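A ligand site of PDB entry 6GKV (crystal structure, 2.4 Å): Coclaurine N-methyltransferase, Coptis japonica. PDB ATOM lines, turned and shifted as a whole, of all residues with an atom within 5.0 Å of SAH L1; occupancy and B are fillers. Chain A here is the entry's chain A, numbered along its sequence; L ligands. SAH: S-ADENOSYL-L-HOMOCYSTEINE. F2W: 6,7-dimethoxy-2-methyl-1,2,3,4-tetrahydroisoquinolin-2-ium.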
ATOM      1  N   VAL A  67       6.561  -7.781 -12.250  1.00  0.00           N
ATOM      2  CA  VAL A  67       6.279  -8.530 -13.483  1.00  0.00           C
ATOM      3  C   VAL A  67       7.390  -9.494 -13.906  1.00  0.00           C
ATOM      4  O   VAL A  67       7.120 -10.653 -14.226  1.00  0.00           O
ATOM      5  CB  VAL A  67       6.016  -7.570 -14.654  1.00  0.00           C
ATOM      6  CG1 VAL A  67       5.592  -8.341 -15.897  1.00  0.00           C
ATOM      7  CG2 VAL A  67       4.986  -6.522 -14.249  1.00  0.00           C
ATOM      8  N   LEU A  70       8.279 -12.022 -11.276  1.00  0.00           N
ATOM      9  CA  LEU A  70       7.271 -13.083 -11.294  1.00  0.00           C
ATOM     10  C   LEU A  70       7.623 -14.113 -12.372  1.00  0.00           C
ATOM     11  O   LEU A  70       7.463 -15.313 -12.161  1.00  0.00           O
ATOM     12  CB  LEU A  70       5.850 -12.534 -11.532  1.00  0.00           C
ATOM     13  CG  LEU A  70       4.676 -13.471 -11.852  1.00  0.00           C
ATOM     14  CD1 LEU A  70       4.563 -14.625 -10.857  1.00  0.00           C
ATOM     15  CD2 LEU A  70       3.363 -12.690 -11.940  1.00  0.00           C
ATOM     16  N   ASP A  71       8.090 -13.628 -13.526  1.00  0.00           N
ATOM     17  CA  ASP A  71       8.524 -14.523 -14.606  1.00  0.00           C
ATOM     18  C   ASP A  71       9.821 -15.264 -14.252  1.00  0.00           C
ATOM     19  O   ASP A  71      10.175 -16.235 -14.911  1.00  0.00           O
ATOM     20  CB  ASP A  71       8.703 -13.746 -15.911  1.00  0.00           C
ATOM     21  CG  ASP A  71       9.049 -14.656 -17.088  1.00  0.00           C
ATOM     22  OD1 ASP A  71       8.152 -15.403 -17.533  1.00  0.00           O
ATOM     23  OD2 ASP A  71      10.200 -14.625 -17.574  1.00  0.00           O
ATOM     24  N   TYR A  75       7.126 -19.634 -13.690  1.00  0.00           N
ATOM     25  CA  TYR A  75       6.852 -19.455 -15.140  1.00  0.00           C
ATOM     26  C   TYR A  75       8.077 -19.494 -16.090  1.00  0.00           C
ATOM     27  O   TYR A  75       7.907 -19.353 -17.313  1.00  0.00           O
ATOM     28  CB  TYR A  75       6.077 -18.144 -15.344  1.00  0.00           C
ATOM     29  CG  TYR A  75       4.742 -18.145 -14.636  1.00  0.00           C
ATOM     30  CD1 TYR A  75       3.971 -19.301 -14.589  1.00  0.00           C
ATOM     31  CD2 TYR A  75       4.289 -17.014 -13.971  1.00  0.00           C
ATOM     32  CE1 TYR A  75       2.765 -19.326 -13.939  1.00  0.00           C
ATOM     33  CE2 TYR A  75       3.080 -17.030 -13.301  1.00  0.00           C
ATOM     34  CZ  TYR A  75       2.323 -18.198 -13.286  1.00  0.00           C
ATOM     35  OH  TYR A  75       1.105 -18.258 -12.642  1.00  0.00           O
ATOM     36  N   LEU A  90       0.221 -30.445 -20.542  1.00  0.00           N
ATOM     37  CA  LEU A  90       0.975 -29.523 -19.720  1.00  0.00           C
ATOM     38  C   LEU A  90       0.090 -28.348 -19.336  1.00  0.00           C
ATOM     39  O   LEU A  90       0.473 -27.179 -19.497  1.00  0.00           O
ATOM     40  CB  LEU A  90       2.221 -29.038 -20.455  1.00  0.00           C
ATOM     41  CG  LEU A  90       3.096 -30.140 -21.071  1.00  0.00           C
ATOM     42  CD1 LEU A  90       4.279 -29.527 -21.792  1.00  0.00           C
ATOM     43  CD2 LEU A  90       3.556 -31.107 -20.007  1.00  0.00           C
ATOM     44  N   LYS A  91      -1.096 -28.660 -18.840  1.00  0.00           N
ATOM     45  CA  LYS A  91      -2.011 -27.634 -18.402  1.00  0.00           C
ATOM     46  C   LYS A  91      -1.656 -27.246 -16.978  1.00  0.00           C
ATOM     47  O   LYS A  91      -1.768 -28.059 -16.069  1.00  0.00           O
ATOM     48  CB  LYS A  91      -3.448 -28.125 -18.490  1.00  0.00           C
ATOM     49  CG  LYS A  91      -4.514 -27.053 -18.244  1.00  0.00           C
ATOM     50  CD  LYS A  91      -5.914 -27.604 -18.478  1.00  0.00           C
ATOM     51  CE  LYS A  91      -6.886 -26.494 -18.825  1.00  0.00           C
ATOM     52  NZ  LYS A  91      -7.077 -25.586 -17.669  1.00  0.00           N
ATOM     53  N   GLY A  92      -1.218 -26.001 -16.787  1.00  0.00           N
ATOM     54  CA  GLY A  92      -0.764 -25.536 -15.501  1.00  0.00           C
ATOM     55  C   GLY A  92      -1.835 -24.715 -14.819  1.00  0.00           C
ATOM     56  O   GLY A  92      -1.554 -23.692 -14.175  1.00  0.00           O
ATOM     57  N   SER A  93      -3.067 -25.182 -14.974  1.00  0.00           N
ATOM     58  CA  SER A  93      -4.259 -24.522 -14.451  1.00  0.00           C
ATOM     59  C   SER A  93      -5.382 -25.564 -14.229  1.00  0.00           C
ATOM     60  O   SER A  93      -5.229 -26.739 -14.601  1.00  0.00           O
ATOM     61  CB  SER A  93      -4.722 -23.432 -15.427  1.00  0.00           C
ATOM     62  OG  SER A  93      -4.808 -23.951 -16.757  1.00  0.00           O
ATOM     63  N   GLY A 131      -1.516 -15.328 -22.014  1.00  0.00           N
ATOM     64  CA  GLY A 131      -0.885 -16.009 -20.913  1.00  0.00           C
ATOM     65  C   GLY A 131      -1.022 -17.502 -21.085  1.00  0.00           C
ATOM     66  O   GLY A 131      -1.565 -18.214 -20.227  1.00  0.00           O
ATOM     67  N   CYS A 132      -0.488 -17.990 -22.201  1.00  0.00           N
ATOM     68  CA  CYS A 132      -0.753 -19.324 -22.717  1.00  0.00           C
ATOM     69  C   CYS A 132      -0.105 -20.504 -21.999  1.00  0.00           C
ATOM     70  O   CYS A 132      -0.406 -21.675 -22.322  1.00  0.00           O
ATOM     71  CB  CYS A 132      -0.303 -19.356 -24.172  1.00  0.00           C
ATOM     72  SG  CYS A 132       1.449 -19.053 -24.328  1.00  0.00           S
ATOM     73  N   GLY A 133       0.789 -20.233 -21.053  1.00  0.00           N
ATOM     74  CA  GLY A 133       1.514 -21.304 -20.386  1.00  0.00           C
ATOM     75  C   GLY A 133       2.325 -22.134 -21.369  1.00  0.00           C
ATOM     76  O   GLY A 133       3.079 -21.587 -22.174  1.00  0.00           O
ATOM     77  N   GLN A 134       2.177 -23.448 -21.303  1.00  0.00           N
ATOM     78  CA  GLN A 134       2.790 -24.337 -22.287  1.00  0.00           C
ATOM     79  C   GLN A 134       1.805 -24.673 -23.411  1.00  0.00           C
ATOM     80  O   GLN A 134       1.933 -25.702 -24.075  1.00  0.00           O
ATOM     81  CB  GLN A 134       3.307 -25.596 -21.622  1.00  0.00           C
ATOM     82  CG  GLN A 134       4.574 -25.373 -20.820  1.00  0.00           C
ATOM     83  CD  GLN A 134       4.323 -24.598 -19.536  1.00  0.00           C
ATOM     84  OE1 GLN A 134       3.252 -24.698 -18.945  1.00  0.00           O
ATOM     85  NE2 GLN A 134       5.315 -23.826 -19.103  1.00  0.00           N
ATOM     86  N   ALA A 136      -1.377 -25.583 -23.660  1.00  0.00           N
ATOM     87  CA  ALA A 136      -2.388 -26.635 -23.579  1.00  0.00           C
ATOM     88  C   ALA A 136      -3.638 -26.267 -24.376  1.00  0.00           C
ATOM     89  O   ALA A 136      -4.182 -27.096 -25.128  1.00  0.00           O
ATOM     90  CB  ALA A 136      -2.740 -26.920 -22.141  1.00  0.00           C
ATOM     91  N   VAL A 153       0.158 -15.669 -26.444  1.00  0.00           N
ATOM     92  CA  VAL A 153       1.015 -14.587 -25.954  1.00  0.00           C
ATOM     93  C   VAL A 153       1.639 -14.873 -24.594  1.00  0.00           C
ATOM     94  O   VAL A 153       0.935 -15.124 -23.626  1.00  0.00           O
ATOM     95  CB  VAL A 153       0.256 -13.272 -25.862  1.00  0.00           C
ATOM     96  CG1 VAL A 153       1.206 -12.169 -25.440  1.00  0.00           C
ATOM     97  CG2 VAL A 153      -0.369 -12.926 -27.186  1.00  0.00           C
ATOM     98  N   THR A 154       2.964 -14.794 -24.529  1.00  0.00           N
ATOM     99  CA  THR A 154       3.720 -15.098 -23.313  1.00  0.00           C
ATOM    100  C   THR A 154       4.865 -14.111 -23.102  1.00  0.00           C
ATOM    101  O   THR A 154       5.397 -13.600 -24.064  1.00  0.00           O
ATOM    102  CB  THR A 154       4.314 -16.493 -23.363  1.00  0.00           C
ATOM    103  OG1 THR A 154       3.334 -17.419 -23.829  1.00  0.00           O
ATOM    104  CG2 THR A 154       4.735 -16.894 -21.998  1.00  0.00           C
ATOM    105  N   ASN A 155       5.244 -13.877 -21.852  1.00  0.00           N
ATOM    106  CA  ASN A 155       6.481 -13.135 -21.575  1.00  0.00           C
ATOM    107  C   ASN A 155       7.594 -14.078 -21.125  1.00  0.00           C
ATOM    108  O   ASN A 155       8.596 -13.650 -20.539  1.00  0.00           O
ATOM    109  CB  ASN A 155       6.228 -12.053 -20.525  1.00  0.00           C
ATOM    110  CG  ASN A 155       5.845 -12.635 -19.168  1.00  0.00           C
ATOM    111  OD1 ASN A 155       5.401 -13.782 -19.069  1.00  0.00           O
ATOM    112  ND2 ASN A 155       5.987 -11.819 -18.120  1.00  0.00           N
ATOM    113  N   SER A 156       7.398 -15.361 -21.399  1.00  0.00           N
ATOM    114  CA  SER A 156       8.272 -16.426 -20.905  1.00  0.00           C
ATOM    115  C   SER A 156       8.987 -17.128 -22.066  1.00  0.00           C
ATOM    116  O   SER A 156       8.372 -17.873 -22.830  1.00  0.00           O
ATOM    117  CB  SER A 156       7.455 -17.428 -20.070  1.00  0.00           C
ATOM    118  OG  SER A 156       8.126 -18.650 -19.868  1.00  0.00           O
ATOM    119  N   GLN A 159       8.245 -20.676 -22.569  1.00  0.00           N
ATOM    120  CA  GLN A 159       6.912 -21.068 -23.026  1.00  0.00           C
ATOM    121  C   GLN A 159       6.742 -20.854 -24.545  1.00  0.00           C
ATOM    122  O   GLN A 159       6.108 -21.669 -25.225  1.00  0.00           O
ATOM    123  CB  GLN A 159       5.838 -20.322 -22.223  1.00  0.00           C
ATOM    124  CG  GLN A 159       5.795 -20.748 -20.756  1.00  0.00           C
ATOM    125  CD  GLN A 159       4.724 -20.036 -19.927  1.00  0.00           C
ATOM    126  OE1 GLN A 159       3.975 -19.211 -20.435  1.00  0.00           O
ATOM    127  NE2 GLN A 159       4.655 -20.368 -18.638  1.00  0.00           N
ATOM    128  N   ALA A 180       5.742 -11.255 -25.286  1.00  0.00           N
ATOM    129  CA  ALA A 180       5.385  -9.892 -24.869  1.00  0.00           C
ATOM    130  C   ALA A 180       4.969  -9.783 -23.396  1.00  0.00           C
ATOM    131  O   ALA A 180       4.404 -10.712 -22.840  1.00  0.00           O
ATOM    132  CB  ALA A 180       4.262  -9.351 -25.745  1.00  0.00           C
ATOM    133  N   ASP A 181       5.265  -8.643 -22.783  1.00  0.00           N
ATOM    134  CA  ASP A 181       4.709  -8.314 -21.475  1.00  0.00           C
ATOM    135  C   ASP A 181       3.313  -7.755 -21.739  1.00  0.00           C
ATOM    136  O   ASP A 181       3.159  -6.706 -22.365  1.00  0.00           O
ATOM    137  CB  ASP A 181       5.599  -7.324 -20.713  1.00  0.00           C
ATOM    138  CG  ASP A 181       5.029  -6.931 -19.341  1.00  0.00           C
ATOM    139  OD1 ASP A 181       4.230  -7.694 -18.764  1.00  0.00           O
ATOM    140  OD2 ASP A 181       5.385  -5.849 -18.829  1.00  0.00           O
ATOM    141  N   ILE A 182       2.285  -8.472 -21.293  1.00  0.00           N
ATOM    142  CA  ILE A 182       0.917  -8.058 -21.552  1.00  0.00           C
ATOM    143  C   ILE A 182       0.630  -6.745 -20.818  1.00  0.00           C
ATOM    144  O   ILE A 182      -0.212  -5.957 -21.271  1.00  0.00           O
ATOM    145  CB  ILE A 182      -0.059  -9.183 -21.142  1.00  0.00           C
ATOM    146  CG1 ILE A 182       0.229 -10.428 -21.976  1.00  0.00           C
ATOM    147  CG2 ILE A 182      -1.519  -8.753 -21.315  1.00  0.00           C
ATOM    148  CD1 ILE A 182      -0.588 -11.649 -21.599  1.00  0.00           C
ATOM    149  N   THR A 183       1.348  -6.508 -19.728  1.00  0.00           N
ATOM    150  CA  THR A 183       1.279  -5.243 -18.987  1.00  0.00           C
ATOM    151  C   THR A 183       1.544  -4.030 -19.887  1.00  0.00           C
ATOM    152  O   THR A 183       0.928  -2.974 -19.740  1.00  0.00           O
ATOM    153  CB  THR A 183       2.291  -5.234 -17.824  1.00  0.00           C
ATOM    154  OG1 THR A 183       1.874  -6.190 -16.851  1.00  0.00           O
ATOM    155  CG2 THR A 183       2.408  -3.859 -17.176  1.00  0.00           C
ATOM    156  N   ILE A 197      -6.816 -17.645 -19.402  1.00  0.00           N
ATOM    157  CA  ILE A 197      -6.924 -18.667 -18.362  1.00  0.00           C
ATOM    158  C   ILE A 197      -5.953 -18.426 -17.201  1.00  0.00           C
ATOM    159  O   ILE A 197      -4.771 -18.761 -17.286  1.00  0.00           O
ATOM    160  CB  ILE A 197      -6.690 -20.075 -18.936  1.00  0.00           C
ATOM    161  CG1 ILE A 197      -7.530 -20.259 -20.192  1.00  0.00           C
ATOM    162  CG2 ILE A 197      -7.028 -21.167 -17.887  1.00  0.00           C
ATOM    163  CD1 ILE A 197      -9.010 -19.977 -19.979  1.00  0.00           C
ATOM    164  N   GLU A 198      -6.482 -17.844 -16.138  1.00  0.00           N
ATOM    165  CA  GLU A 198      -5.766 -17.676 -14.869  1.00  0.00           C
ATOM    166  C   GLU A 198      -4.539 -16.798 -15.060  1.00  0.00           C
ATOM    167  O   GLU A 198      -3.435 -17.208 -14.803  1.00  0.00           O
ATOM    168  CB  GLU A 198      -5.401 -19.039 -14.259  1.00  0.00           C
ATOM    169  CG  GLU A 198      -6.627 -19.831 -13.826  1.00  0.00           C
ATOM    170  CD  GLU A 198      -6.316 -21.120 -13.087  1.00  0.00           C
ATOM    171  OE1 GLU A 198      -5.191 -21.265 -12.554  1.00  0.00           O
ATOM    172  OE2 GLU A 198      -7.194 -22.004 -13.062  1.00  0.00           O
ATOM    173  N   LEU A 199      -4.778 -15.567 -15.502  1.00  0.00           N
ATOM    174  CA  LEU A 199      -3.722 -14.596 -15.719  1.00  0.00           C
ATOM    175  C   LEU A 199      -3.893 -13.398 -14.806  1.00  0.00           C
ATOM    176  O   LEU A 199      -2.921 -12.884 -14.248  1.00  0.00           O
ATOM    177  CB  LEU A 199      -3.709 -14.130 -17.173  1.00  0.00           C
ATOM    178  CG  LEU A 199      -2.794 -12.948 -17.483  1.00  0.00           C
ATOM    179  CD1 LEU A 199      -1.331 -13.371 -17.461  1.00  0.00           C
ATOM    180  CD2 LEU A 199      -3.171 -12.305 -18.810  1.00  0.00           C
ATOM    181  N   HIS A 202      -2.373 -12.336 -11.319  1.00  0.00           N
ATOM    182  CA  HIS A 202      -1.038 -11.711 -11.288  1.00  0.00           C
ATOM    183  C   HIS A 202      -1.071 -10.233 -11.612  1.00  0.00           C
ATOM    184  O   HIS A 202      -0.065  -9.535 -11.514  1.00  0.00           O
ATOM    185  CB  HIS A 202      -0.133 -12.417 -12.292  1.00  0.00           C
ATOM    186  CG  HIS A 202       0.079 -13.865 -11.996  1.00  0.00           C
ATOM    187  ND1 HIS A 202       0.580 -14.309 -10.780  1.00  0.00           N
ATOM    188  CD2 HIS A 202      -0.111 -14.964 -12.749  1.00  0.00           C
ATOM    189  CE1 HIS A 202       0.680 -15.626 -10.808  1.00  0.00           C
ATOM    190  NE2 HIS A 202       0.266 -16.044 -11.994  1.00  0.00           N
ATOM    191  N   MET A 203      -2.248  -9.759 -12.030  1.00  0.00           N
ATOM    192  CA  MET A 203      -2.409  -8.367 -12.428  1.00  0.00           C
ATOM    193  C   MET A 203      -2.967  -7.588 -11.260  1.00  0.00           C
ATOM    194  O   MET A 203      -3.251  -8.151 -10.222  1.00  0.00           O
ATOM    195  CB  MET A 203      -3.333  -8.254 -13.641  1.00  0.00           C
ATOM    196  CG  MET A 203      -2.953  -9.171 -14.776  1.00  0.00           C
ATOM    197  SD  MET A 203      -1.349  -8.763 -15.510  1.00  0.00           S
ATOM    198  CE  MET A 203      -0.532 -10.364 -15.471  1.00  0.00           C
HETATM  199  N   SAH L   1      -2.798 -20.145 -19.145  1.00  0.00           N
HETATM  200  CA  SAH L   1      -1.845 -21.221 -18.919  1.00  0.00           C
HETATM  201  CB  SAH L   1      -0.966 -20.925 -17.719  1.00  0.00           C
HETATM  202  CG  SAH L   1      -1.621 -20.146 -16.587  1.00  0.00           C
HETATM  203  SD  SAH L   1      -0.390 -19.658 -15.335  1.00  0.00           S
HETATM  204  C   SAH L   1      -2.555 -22.560 -18.707  1.00  0.00           C
HETATM  205  O   SAH L   1      -3.759 -22.550 -18.449  1.00  0.00           O
HETATM  206  OXT SAH L   1      -1.940 -23.640 -18.795  1.00  0.00           O
HETATM  207  C5' SAH L   1      -0.350 -17.927 -15.870  1.00  0.00           C
HETATM  208  C4' SAH L   1       0.254 -17.713 -17.271  1.00  0.00           C
HETATM  209  O4' SAH L   1       0.291 -16.325 -17.576  1.00  0.00           O
HETATM  210  C3' SAH L   1       1.679 -18.215 -17.375  1.00  0.00           C
HETATM  211  O3' SAH L   1       1.879 -18.757 -18.662  1.00  0.00           O
HETATM  212  C2' SAH L   1       2.546 -16.991 -17.279  1.00  0.00           C
HETATM  213  O2' SAH L   1       3.704 -17.180 -18.065  1.00  0.00           O
HETATM  214  C1' SAH L   1       1.625 -15.914 -17.853  1.00  0.00           C
HETATM  215  N9  SAH L   1       1.885 -14.562 -17.296  1.00  0.00           N
HETATM  216  C8  SAH L   1       1.963 -14.172 -15.983  1.00  0.00           C
HETATM  217  N7  SAH L   1       2.228 -12.838 -15.941  1.00  0.00           N
HETATM  218  C5  SAH L   1       2.307 -12.370 -17.221  1.00  0.00           C
HETATM  219  C6  SAH L   1       2.563 -11.110 -17.769  1.00  0.00           C
HETATM  220  N6  SAH L   1       2.776 -10.047 -16.988  1.00  0.00           N
HETATM  221  N1  SAH L   1       2.581 -10.952 -19.147  1.00  0.00           N
HETATM  222  C2  SAH L   1       2.371 -12.047 -19.967  1.00  0.00           C
HETATM  223  N3  SAH L   1       2.126 -13.294 -19.419  1.00  0.00           N
HETATM  224  C4  SAH L   1       2.094 -13.447 -18.079  1.00  0.00           C
HETATM  225  CAM F2W L   2      -1.729 -24.171  -6.123  1.00  0.00           C
HETATM  226  OAK F2W L   2      -2.440 -22.969  -5.732  1.00  0.00           O
HETATM  227  CAB F2W L   2      -2.605 -22.139  -6.818  1.00  0.00           C
HETATM  228  CAA F2W L   2      -2.185 -22.467  -8.103  1.00  0.00           C
HETATM  229  CAF F2W L   2      -2.392 -21.541  -9.119  1.00  0.00           C
HETATM  230  CAJ F2W L   2      -2.042 -21.794 -10.436  1.00  0.00           C
HETATM  231  CAI F2W L   2      -1.819 -20.560 -11.380  1.00  0.00           C
HETATM  232  NAH F2W L   2      -3.096 -19.835 -11.336  1.00  0.00           N
HETATM  233  CAO F2W L   2      -2.750 -18.566 -12.001  1.00  0.00           C
HETATM  234  CAG F2W L   2      -3.139 -19.496  -9.920  1.00  0.00           C
HETATM  235  CAE F2W L   2      -3.073 -20.378  -8.885  1.00  0.00           C
HETATM  236  CAD F2W L   2      -3.464 -20.045  -7.589  1.00  0.00           C
HETATM  237  CAC F2W L   2      -3.265 -20.948  -6.569  1.00  0.00           C
HETATM  238  OAL F2W L   2      -3.616 -20.725  -5.264  1.00  0.00           O
HETATM  239  CAN F2W L   2      -4.308 -19.508  -4.922  1.00  0.00           C
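An oxygen (O) of SAH L1 sits at hydrogen-bond distance from the side-chain hydroxyl of Ser 93, 2.4 Å away.
OXT of SAH L1 lies within hydrogen-bond range of N of Gly 92, 3.2 Å away.
O of Ile 197 is in hydrogen-bond range of N of SAH L1 (3.0 Å).
N of Ile 182 is in hydrogen-bond range of N1 of SAH L1.
SD of SAH L1 sits close to OH of Tyr 75, 3.4 Å away.
O3' of SAH L1 lies within hydrogen-bond range of OE1 of Gln 159, at 2.8 Å.
O of Gly 131 is in hydrogen-bond range of N of SAH L1, at 2.5 Å.
OD1 of Asn 155 lies close to N3 of SAH L1 (3.3 Å).
An oxygen (O3') of SAH L1 is in hydrogen-bond range of the backbone NH of Gly 133, at 3.0 Å.
The side-chain carboxylate (OD1) of Asp 181 sits at hydrogen-bond distance from a nitrogen (N6) of SAH L1 (3.3 Å).
OE1 of Glu 198 is in salt-bridge range of NAH of F2W L2 (2.8 Å).
OE1 of Gln 159 sits close to O of Gly 133, 3.1 Å away.
The backbone NH of Gln 159 sits close to the side-chain hydroxyl of Ser 156, at 3.4 Å.
O of Tyr 75 lies within hydrogen-bond range of OG of Ser 156.
The side-chain hydroxyl (OG1) of Thr 154 is in hydrogen-bond range of the side-chain sulfur (SG) of Cys 132 (2.5 Å).
The backbone NH (N) of Gly 131 is in hydrogen-bond range of the backbone carbonyl oxygen (O) of Val 153, at 2.9 Å.
The backbone carbonyl oxygen (O) of Ala 180 lies close to the backbone NH (N) of Asn 155, at 3.4 Å.
NE2 of His 202 lies within hydrogen-bond range of OH of Tyr 75.
The side-chain amino group (NZ) of Lys 91 sits at hydrogen-bond distance from the side-chain hydroxyl (OG) of Ser 93, 2.9 Å away.
Val 67 touches SAH L1 (CG1 to N6, 3.5 Å).
Cys 132 touches SAH L1 (C to CA, 3.6 Å).
Ala 180 touches SAH L1.
Thr 183 touches SAH L1 (OG1 to N6, 3.96 Å).
O of Glu 198 touches C5' of SAH L1, at 3.3 Å.
Leu 199 touches SAH L1 (CD1 to O4', 3.4 Å).
His 202 touches SAH L1 (CD2 to C8, 3.9 Å).
Met 203 touches SAH L1.
Within 4 Å of SAH L1: Val 67, Tyr 75, Gly 92, Ser 93, Gly 131, Cys 132, Gly 133, Asn 155, Gln 159, Ala 180, Asp 181, Ile 182, Thr 183, Ile 197, Glu 198, Leu 199, His 202 and Met 203.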
